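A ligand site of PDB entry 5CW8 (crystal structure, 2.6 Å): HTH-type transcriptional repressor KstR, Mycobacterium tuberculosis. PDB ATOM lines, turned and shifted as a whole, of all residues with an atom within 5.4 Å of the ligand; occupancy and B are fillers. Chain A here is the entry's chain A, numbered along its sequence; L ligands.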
ATOM      1  N   MET A  30      10.051 -12.075 -16.078  1.00  0.00           N
ATOM      2  CA  MET A  30      11.065 -12.071 -17.121  1.00  0.00           C
ATOM      3  C   MET A  30      11.094 -10.759 -17.911  1.00  0.00           C
ATOM      4  O   MET A  30      12.166 -10.218 -18.178  1.00  0.00           O
ATOM      5  CB  MET A  30      10.841 -13.251 -18.079  1.00  0.00           C
ATOM      6  CG  MET A  30      11.197 -14.596 -17.481  1.00  0.00           C
ATOM      7  SD  MET A  30      12.974 -14.757 -17.186  1.00  0.00           S
ATOM      8  CE  MET A  30      13.580 -14.700 -18.870  1.00  0.00           C
ATOM      9  N   SER A  34      14.073  -8.093 -17.682  1.00  0.00           N
ATOM     10  CA  SER A  34      14.762  -7.858 -18.948  1.00  0.00           C
ATOM     11  C   SER A  34      14.804  -6.378 -19.279  1.00  0.00           C
ATOM     12  O   SER A  34      15.787  -5.901 -19.855  1.00  0.00           O
ATOM     13  CB  SER A  34      14.087  -8.640 -20.088  1.00  0.00           C
ATOM     14  OG  SER A  34      14.267 -10.030 -19.922  1.00  0.00           O
ATOM     15  N   LEU A  72      14.159 -18.245 -14.047  1.00  0.00           N
ATOM     16  CA  LEU A  72      15.380 -18.852 -14.569  1.00  0.00           C
ATOM     17  C   LEU A  72      15.219 -20.362 -14.774  1.00  0.00           C
ATOM     18  O   LEU A  72      15.618 -20.904 -15.804  1.00  0.00           O
ATOM     19  CB  LEU A  72      16.551 -18.576 -13.628  1.00  0.00           C
ATOM     20  CG  LEU A  72      17.905 -19.097 -14.102  1.00  0.00           C
ATOM     21  CD1 LEU A  72      18.372 -18.347 -15.343  1.00  0.00           C
ATOM     22  CD2 LEU A  72      18.932 -19.011 -12.982  1.00  0.00           C
ATOM     23  N   GLU A  75      13.059 -21.107 -17.730  1.00  0.00           N
ATOM     24  CA  GLU A  75      13.821 -20.825 -18.940  1.00  0.00           C
ATOM     25  C   GLU A  75      14.794 -21.950 -19.251  1.00  0.00           C
ATOM     26  O   GLU A  75      14.981 -22.305 -20.410  1.00  0.00           O
ATOM     27  CB  GLU A  75      14.558 -19.492 -18.819  1.00  0.00           C
ATOM     28  CG  GLU A  75      14.270 -18.526 -19.958  1.00  0.00           C
ATOM     29  CD  GLU A  75      12.786 -18.281 -20.162  1.00  0.00           C
ATOM     30  OE1 GLU A  75      12.338 -18.247 -21.321  1.00  0.00           O
ATOM     31  OE2 GLU A  75      12.064 -18.116 -19.151  1.00  0.00           O
ATOM     32  N   PHE A  76      15.423 -22.515 -18.219  1.00  0.00           N
ATOM     33  CA  PHE A  76      16.333 -23.638 -18.412  1.00  0.00           C
ATOM     34  C   PHE A  76      15.592 -24.869 -18.906  1.00  0.00           C
ATOM     35  O   PHE A  76      16.024 -25.526 -19.855  1.00  0.00           O
ATOM     36  CB  PHE A  76      17.079 -23.956 -17.115  1.00  0.00           C
ATOM     37  CG  PHE A  76      18.247 -23.060 -16.838  1.00  0.00           C
ATOM     38  CD1 PHE A  76      18.763 -22.254 -17.838  1.00  0.00           C
ATOM     39  CD2 PHE A  76      18.831 -23.022 -15.584  1.00  0.00           C
ATOM     40  CE1 PHE A  76      19.836 -21.423 -17.588  1.00  0.00           C
ATOM     41  CE2 PHE A  76      19.911 -22.198 -15.330  1.00  0.00           C
ATOM     42  CZ  PHE A  76      20.410 -21.395 -16.334  1.00  0.00           C
ATOM     43  N   ILE A  79      14.819 -24.358 -22.446  1.00  0.00           N
ATOM     44  CA  ILE A  79      16.019 -24.497 -23.258  1.00  0.00           C
ATOM     45  C   ILE A  79      16.288 -25.988 -23.483  1.00  0.00           C
ATOM     46  O   ILE A  79      16.755 -26.387 -24.560  1.00  0.00           O
ATOM     47  CB  ILE A  79      17.238 -23.801 -22.614  1.00  0.00           C
ATOM     48  CG1 ILE A  79      17.133 -22.276 -22.759  1.00  0.00           C
ATOM     49  CG2 ILE A  79      18.542 -24.300 -23.214  1.00  0.00           C
ATOM     50  CD1 ILE A  79      17.222 -21.794 -24.194  1.00  0.00           C
ATOM     51  N   LEU A 104      24.368 -21.345 -23.753  1.00  0.00           N
ATOM     52  CA  LEU A 104      24.011 -20.598 -22.549  1.00  0.00           C
ATOM     53  C   LEU A 104      24.813 -19.311 -22.405  1.00  0.00           C
ATOM     54  O   LEU A 104      24.323 -18.306 -21.892  1.00  0.00           O
ATOM     55  CB  LEU A 104      24.216 -21.483 -21.308  1.00  0.00           C
ATOM     56  CG  LEU A 104      23.262 -22.673 -21.183  1.00  0.00           C
ATOM     57  CD1 LEU A 104      23.575 -23.486 -19.945  1.00  0.00           C
ATOM     58  CD2 LEU A 104      21.812 -22.196 -21.162  1.00  0.00           C
ATOM     59  N   ALA A 107      23.470 -16.773 -24.819  1.00  0.00           N
ATOM     60  CA  ALA A 107      22.236 -16.285 -24.222  1.00  0.00           C
ATOM     61  C   ALA A 107      22.522 -15.250 -23.131  1.00  0.00           C
ATOM     62  O   ALA A 107      21.868 -14.211 -23.064  1.00  0.00           O
ATOM     63  CB  ALA A 107      21.434 -17.446 -23.653  1.00  0.00           C
ATOM     64  N   MET A 108      23.509 -15.540 -22.278  1.00  0.00           N
ATOM     65  CA  MET A 108      23.915 -14.615 -21.225  1.00  0.00           C
ATOM     66  C   MET A 108      24.320 -13.275 -21.806  1.00  0.00           C
ATOM     67  O   MET A 108      23.847 -12.225 -21.364  1.00  0.00           O
ATOM     68  CB  MET A 108      25.066 -15.189 -20.408  1.00  0.00           C
ATOM     69  CG  MET A 108      25.685 -14.156 -19.458  1.00  0.00           C
ATOM     70  SD  MET A 108      27.164 -14.731 -18.612  1.00  0.00           S
ATOM     71  CE  MET A 108      28.278 -14.952 -19.993  1.00  0.00           C
ATOM     72  N   ASN A 111      21.610 -10.908 -23.071  1.00  0.00           N
ATOM     73  CA  ASN A 111      20.655 -10.358 -22.122  1.00  0.00           C
ATOM     74  C   ASN A 111      21.328  -9.857 -20.842  1.00  0.00           C
ATOM     75  O   ASN A 111      21.182 -10.465 -19.786  1.00  0.00           O
ATOM     76  CB  ASN A 111      19.604 -11.404 -21.757  1.00  0.00           C
ATOM     77  CG  ASN A 111      18.860 -11.935 -22.958  1.00  0.00           C
ATOM     78  OD1 ASN A 111      17.866 -11.356 -23.399  1.00  0.00           O
ATOM     79  ND2 ASN A 111      19.347 -13.037 -23.519  1.00  0.00           N
ATOM     80  N   LEU A 114      18.933  -8.904 -17.704  1.00  0.00           N
ATOM     81  CA  LEU A 114      18.358 -10.133 -17.173  1.00  0.00           C
ATOM     82  C   LEU A 114      19.402 -10.920 -16.401  1.00  0.00           C
ATOM     83  O   LEU A 114      19.128 -11.489 -15.333  1.00  0.00           O
ATOM     84  CB  LEU A 114      17.779 -10.972 -18.307  1.00  0.00           C
ATOM     85  CG  LEU A 114      17.178 -12.331 -17.931  1.00  0.00           C
ATOM     86  CD1 LEU A 114      15.966 -12.143 -17.030  1.00  0.00           C
ATOM     87  CD2 LEU A 114      16.821 -13.100 -19.191  1.00  0.00           C
ATOM     88  N   THR A 115      20.618 -10.950 -16.938  1.00  0.00           N
ATOM     89  CA  THR A 115      21.741 -11.623 -16.294  1.00  0.00           C
ATOM     90  C   THR A 115      22.078 -10.936 -14.966  1.00  0.00           C
ATOM     91  O   THR A 115      22.401 -11.602 -13.985  1.00  0.00           O
ATOM     92  CB  THR A 115      22.986 -11.624 -17.199  1.00  0.00           C
ATOM     93  OG1 THR A 115      22.683 -12.327 -18.415  1.00  0.00           O
ATOM     94  CG2 THR A 115      24.158 -12.307 -16.503  1.00  0.00           C
ATOM     95  N   MET A 118      19.358 -12.061 -12.498  1.00  0.00           N
ATOM     96  CA  MET A 118      19.581 -13.439 -12.054  1.00  0.00           C
ATOM     97  C   MET A 118      20.767 -13.560 -11.100  1.00  0.00           C
ATOM     98  O   MET A 118      20.666 -14.213 -10.061  1.00  0.00           O
ATOM     99  CB  MET A 118      19.803 -14.371 -13.244  1.00  0.00           C
ATOM    100  CG  MET A 118      18.591 -14.517 -14.141  1.00  0.00           C
ATOM    101  SD  MET A 118      17.100 -14.971 -13.233  1.00  0.00           S
ATOM    102  CE  MET A 118      15.905 -15.005 -14.538  1.00  0.00           C
ATOM    103  N   TYR A 122      20.855 -14.703  -7.206  1.00  0.00           N
ATOM    104  CA  TYR A 122      21.642 -15.789  -6.644  1.00  0.00           C
ATOM    105  C   TYR A 122      22.536 -15.297  -5.511  1.00  0.00           C
ATOM    106  O   TYR A 122      22.854 -16.059  -4.594  1.00  0.00           O
ATOM    107  CB  TYR A 122      22.498 -16.448  -7.726  1.00  0.00           C
ATOM    108  CG  TYR A 122      21.877 -17.710  -8.254  1.00  0.00           C
ATOM    109  CD1 TYR A 122      22.220 -18.950  -7.734  1.00  0.00           C
ATOM    110  CD2 TYR A 122      20.928 -17.665  -9.271  1.00  0.00           C
ATOM    111  CE1 TYR A 122      21.642 -20.104  -8.212  1.00  0.00           C
ATOM    112  CE2 TYR A 122      20.343 -18.813  -9.753  1.00  0.00           C
ATOM    113  CZ  TYR A 122      20.708 -20.035  -9.216  1.00  0.00           C
ATOM    114  OH  TYR A 122      20.131 -21.181  -9.705  1.00  0.00           O
ATOM    115  N   VAL A 136      16.792 -25.433  -9.829  1.00  0.00           N
ATOM    116  CA  VAL A 136      17.577 -24.897 -10.927  1.00  0.00           C
ATOM    117  C   VAL A 136      18.848 -25.733 -11.080  1.00  0.00           C
ATOM    118  O   VAL A 136      19.188 -26.152 -12.188  1.00  0.00           O
ATOM    119  CB  VAL A 136      17.908 -23.407 -10.742  1.00  0.00           C
ATOM    120  CG1 VAL A 136      18.815 -22.932 -11.855  1.00  0.00           C
ATOM    121  CG2 VAL A 136      16.630 -22.601 -10.738  1.00  0.00           C
ATOM    122  N   GLU A 137      19.530 -25.981  -9.955  1.00  0.00           N
ATOM    123  CA  GLU A 137      20.761 -26.770  -9.958  1.00  0.00           C
ATOM    124  C   GLU A 137      20.557 -28.054 -10.732  1.00  0.00           C
ATOM    125  O   GLU A 137      21.146 -28.243 -11.814  1.00  0.00           O
ATOM    126  CB  GLU A 137      21.229 -27.090  -8.539  1.00  0.00           C
ATOM    127  CG  GLU A 137      22.111 -26.034  -7.912  1.00  0.00           C
ATOM    128  CD  GLU A 137      22.822 -26.546  -6.666  1.00  0.00           C
ATOM    129  OE1 GLU A 137      23.305 -27.694  -6.694  1.00  0.00           O
ATOM    130  OE2 GLU A 137      22.887 -25.799  -5.659  1.00  0.00           O
ATOM    131  N   ILE A 140      20.219 -27.434 -14.533  1.00  0.00           N
ATOM    132  CA  ILE A 140      21.329 -27.009 -15.369  1.00  0.00           C
ATOM    133  C   ILE A 140      22.418 -28.077 -15.328  1.00  0.00           C
ATOM    134  O   ILE A 140      22.982 -28.443 -16.359  1.00  0.00           O
ATOM    135  CB  ILE A 140      21.846 -25.602 -14.957  1.00  0.00           C
ATOM    136  CG1 ILE A 140      22.897 -25.094 -15.952  1.00  0.00           C
ATOM    137  CG2 ILE A 140      22.381 -25.588 -13.532  1.00  0.00           C
ATOM    138  N   ASP A 141      22.678 -28.616 -14.137  1.00  0.00           N
ATOM    139  CA  ASP A 141      23.620 -29.718 -13.979  1.00  0.00           C
ATOM    140  C   ASP A 141      23.247 -30.880 -14.878  1.00  0.00           C
ATOM    141  O   ASP A 141      24.110 -31.424 -15.595  1.00  0.00           O
ATOM    142  CB  ASP A 141      23.675 -30.175 -12.510  1.00  0.00           C
ATOM    143  CG  ASP A 141      24.612 -29.330 -11.676  1.00  0.00           C
ATOM    144  OD1 ASP A 141      25.002 -28.228 -12.127  1.00  0.00           O
ATOM    145  OD2 ASP A 141      24.966 -29.760 -10.551  1.00  0.00           O
ATOM    146  N   PHE A 144      24.059 -30.212 -18.297  1.00  0.00           N
ATOM    147  CA  PHE A 144      25.472 -30.336 -18.568  1.00  0.00           C
ATOM    148  C   PHE A 144      25.842 -31.821 -18.609  1.00  0.00           C
ATOM    149  O   PHE A 144      26.523 -32.278 -19.530  1.00  0.00           O
ATOM    150  CB  PHE A 144      26.300 -29.595 -17.525  1.00  0.00           C
ATOM    151  CG  PHE A 144      26.250 -28.097 -17.651  1.00  0.00           C
ATOM    152  CD1 PHE A 144      26.057 -27.505 -18.883  1.00  0.00           C
ATOM    153  CD2 PHE A 144      26.383 -27.289 -16.537  1.00  0.00           C
ATOM    154  CE1 PHE A 144      26.009 -26.119 -18.994  1.00  0.00           C
ATOM    155  CE2 PHE A 144      26.328 -25.906 -16.642  1.00  0.00           C
ATOM    156  CZ  PHE A 144      26.148 -25.318 -17.876  1.00  0.00           C
ATOM    157  N   ARG A 162      28.566 -29.406 -11.807  1.00  0.00           N
ATOM    158  CA  ARG A 162      28.527 -28.518 -10.648  1.00  0.00           C
ATOM    159  C   ARG A 162      29.739 -27.591 -10.594  1.00  0.00           C
ATOM    160  O   ARG A 162      29.628 -26.413 -10.233  1.00  0.00           O
ATOM    161  CB  ARG A 162      28.420 -29.330  -9.353  1.00  0.00           C
ATOM    162  CG  ARG A 162      28.255 -28.497  -8.094  1.00  0.00           C
ATOM    163  CD  ARG A 162      26.788 -28.332  -7.707  1.00  0.00           C
ATOM    164  NE  ARG A 162      25.988 -27.685  -8.739  1.00  0.00           N
ATOM    165  CZ  ARG A 162      25.822 -26.361  -8.839  1.00  0.00           C
ATOM    166  NH1 ARG A 162      26.408 -25.544  -7.978  1.00  0.00           N
ATOM    167  NH2 ARG A 162      25.066 -25.860  -9.807  1.00  0.00           N
ATOM    168  N   SER A 165      29.182 -24.849 -13.105  1.00  0.00           N
ATOM    169  CA  SER A 165      28.225 -23.896 -12.566  1.00  0.00           C
ATOM    170  C   SER A 165      28.862 -22.984 -11.522  1.00  0.00           C
ATOM    171  O   SER A 165      28.497 -21.806 -11.392  1.00  0.00           O
ATOM    172  CB  SER A 165      27.032 -24.624 -11.965  1.00  0.00           C
ATOM    173  OG  SER A 165      26.528 -25.614 -12.857  1.00  0.00           O
ATOM    174  N   TRP A 168      31.111 -20.487 -13.239  1.00  0.00           N
ATOM    175  CA  TRP A 168      30.155 -19.551 -13.826  1.00  0.00           C
ATOM    176  C   TRP A 168      29.677 -18.518 -12.807  1.00  0.00           C
ATOM    177  O   TRP A 168      29.676 -17.317 -13.075  1.00  0.00           O
ATOM    178  CB  TRP A 168      28.956 -20.298 -14.391  1.00  0.00           C
ATOM    179  CG  TRP A 168      28.344 -19.637 -15.582  1.00  0.00           C
ATOM    180  CD1 TRP A 168      28.043 -18.307 -15.708  1.00  0.00           C
ATOM    181  CD2 TRP A 168      27.971 -20.260 -16.810  1.00  0.00           C
ATOM    182  NE1 TRP A 168      27.512 -18.068 -16.950  1.00  0.00           N
ATOM    183  CE2 TRP A 168      27.445 -19.241 -17.643  1.00  0.00           C
ATOM    184  CE3 TRP A 168      28.016 -21.570 -17.292  1.00  0.00           C
ATOM    185  CZ2 TRP A 168      26.981 -19.509 -18.927  1.00  0.00           C
ATOM    186  CZ3 TRP A 168      27.557 -21.824 -18.563  1.00  0.00           C
ATOM    187  CH2 TRP A 168      27.049 -20.804 -19.374  1.00  0.00           C
ATOM    188  N   LEU A 169      29.280 -18.995 -11.631  1.00  0.00           N
ATOM    189  CA  LEU A 169      28.699 -18.120 -10.627  1.00  0.00           C
ATOM    190  C   LEU A 169      29.733 -17.186 -10.009  1.00  0.00           C
ATOM    191  O   LEU A 169      29.456 -16.009  -9.777  1.00  0.00           O
ATOM    192  CB  LEU A 169      28.017 -18.941  -9.524  1.00  0.00           C
ATOM    193  CG  LEU A 169      27.365 -18.096  -8.440  1.00  0.00           C
ATOM    194  CD1 LEU A 169      26.343 -17.123  -9.039  1.00  0.00           C
ATOM    195  CD2 LEU A 169      26.718 -18.981  -7.390  1.00  0.00           C
ATOM    196  N   LEU A 172      30.639 -14.615 -12.499  1.00  0.00           N
ATOM    197  CA  LEU A 172      29.493 -13.719 -12.573  1.00  0.00           C
ATOM    198  C   LEU A 172      29.469 -12.755 -11.394  1.00  0.00           C
ATOM    199  O   LEU A 172      29.003 -11.631 -11.517  1.00  0.00           O
ATOM    200  CB  LEU A 172      28.172 -14.495 -12.637  1.00  0.00           C
ATOM    201  CG  LEU A 172      27.704 -14.918 -14.028  1.00  0.00           C
ATOM    202  CD1 LEU A 172      26.457 -15.762 -13.910  1.00  0.00           C
ATOM    203  CD2 LEU A 172      27.463 -13.713 -14.909  1.00  0.00           C
HETATM  204  C1  LIG L   1      15.696 -13.930 -22.824  1.00  0.00           C
HETATM  205  S1  LIG L   1      15.545 -15.628 -22.176  1.00  0.00           S
HETATM  206  C2  LIG L   1      17.200 -16.159 -22.320  1.00  0.00           C
HETATM  207  C3  LIG L   1      17.757 -16.925 -21.113  1.00  0.00           C
HETATM  208  C4  LIG L   1      19.225 -16.541 -20.944  1.00  0.00           C
HETATM  209  C5  LIG L   1      19.588 -16.335 -19.470  1.00  0.00           C
HETATM  210  C6  LIG L   1      21.076 -15.958 -19.410  1.00  0.00           C
HETATM  211  C7  LIG L   1      23.352 -20.027 -11.755  1.00  0.00           C
HETATM  212  C8  LIG L   1      23.808 -21.040 -10.698  1.00  0.00           C
HETATM  213  C9  LIG L   1      23.106 -17.987 -13.938  1.00  0.00           C
HETATM  214  C10 LIG L   1      23.510 -19.204 -17.987  1.00  0.00           C
HETATM  215  C11 LIG L   1      22.534 -18.256 -18.687  1.00  0.00           C
HETATM  216  C12 LIG L   1      20.617 -15.314 -17.044  1.00  0.00           C
HETATM  217  C13 LIG L   1      21.607 -16.021 -17.976  1.00  0.00           C
HETATM  218  C14 LIG L   1      24.678 -21.400 -13.352  1.00  0.00           C
HETATM  219  C15 LIG L   1      24.239 -20.081 -13.020  1.00  0.00           C
HETATM  220  C16 LIG L   1      25.474 -19.212 -12.789  1.00  0.00           C
HETATM  221  C17 LIG L   1      22.746 -17.694 -16.379  1.00  0.00           C
HETATM  222  C18 LIG L   1      24.026 -16.852 -16.525  1.00  0.00           C
HETATM  223  C19 LIG L   1      23.988 -22.335 -11.239  1.00  0.00           C
HETATM  224  O1  LIG L   1      23.846 -23.331 -10.532  1.00  0.00           O
HETATM  225  C20 LIG L   1      24.253 -21.133 -15.737  1.00  0.00           C
HETATM  226  C21 LIG L   1      24.022 -19.660 -15.525  1.00  0.00           C
HETATM  227  C22 LIG L   1      23.388 -19.481 -14.165  1.00  0.00           C
HETATM  228  C23 LIG L   1      23.021 -19.162 -16.555  1.00  0.00           C
HETATM  229  C24 LIG L   1      21.808 -17.488 -17.564  1.00  0.00           C
HETATM  230  C25 LIG L   1      22.138 -17.481 -15.006  1.00  0.00           C
HETATM  231  C26 LIG L   1      24.339 -22.510 -12.574  1.00  0.00           C
HETATM  232  C27 LIG L   1      25.154 -21.683 -14.639  1.00  0.00           C
HETATM  233  O2  LIG L   1      17.905 -15.955 -23.311  1.00  0.00           O
HETATM  234  C28 LIG L   1      17.643 -18.422 -21.368  1.00  0.00           C
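Residues that only touch the ligand: Met 30 (3.96 Å), Leu 72 (3.9 Å), Glu 75 (3.7 Å), Phe 76 (3.4 Å), Leu 104 (3.7 Å), Ala 107 (3.6 Å), Met 108 (3.6 Å), Leu 114 (3.9 Å), Thr 115 (3.9 Å), Met 118 (3.6 Å), Tyr 122 (3.4 Å), Ile 140 (3.8 Å), Ser 165 (3.5 Å), Trp 168 (3.6 Å), Leu 169 (3.98 Å) and Leu 172 (3.7 Å). Hydrophobic or aromatic side chains within 4 Å of the ligand: Met 30, Leu 72, Phe 76, Ala 107, Leu 114, Met 118, Tyr 122, Ile 140, Trp 168 and Leu 172. Within 4 Å of the ligand: Met 30, Leu 72, Glu 75, Phe 76, Leu 104, Ala 107, Met 108, Asn 111, Leu 114, Thr 115, Met 118, Tyr 122, Ile 140, Arg 162, Ser 165, Trp 168, Leu 169 and Leu 172. The nearest printed residue that does not touch the ligand is Ile 79 (4.1 Å).
An oxygen (O2) of the ligand lies within hydrogen-bond range of the side-chain amide nitrogen (ND2) of Asn 111, at 3.3 Å. NH2 of Arg 162 is in hydrogen-bond range of O1 of the ligand, 2.9 Å away.
The backbone carbonyl oxygen (O) of Met 30 is in hydrogen-bond range of the side-chain hydroxyl (OG) of Ser 34. The backbone carbonyl oxygen of Met 108 lies within hydrogen-bond range of the side-chain hydroxyl of Thr 115 (3.2 Å). OE1 of Glu 137 lies within salt-bridge range of NE of Arg 162. The guanidinium group (NE) of Arg 162 is in salt-bridge range of the side-chain carboxylate (OD2) of Asp 141 (2.9 Å). The guanidinium group (NH2) of Arg 162 lies close to the side-chain hydroxyl (OG) of Ser 165, at 3.4 Å. The side-chain hydroxyl (OG) of Ser 165 sits at hydrogen-bond distance from the side-chain carboxylate (OD1) of Asp 141. O of Ala 107 lies within hydrogen-bond range of ND2 of Asn 111. The backbone carbonyl oxygen (O) of Asn 111 sits at hydrogen-bond distance from the side-chain hydroxyl (OG1) of Thr 115 (2.8 Å).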
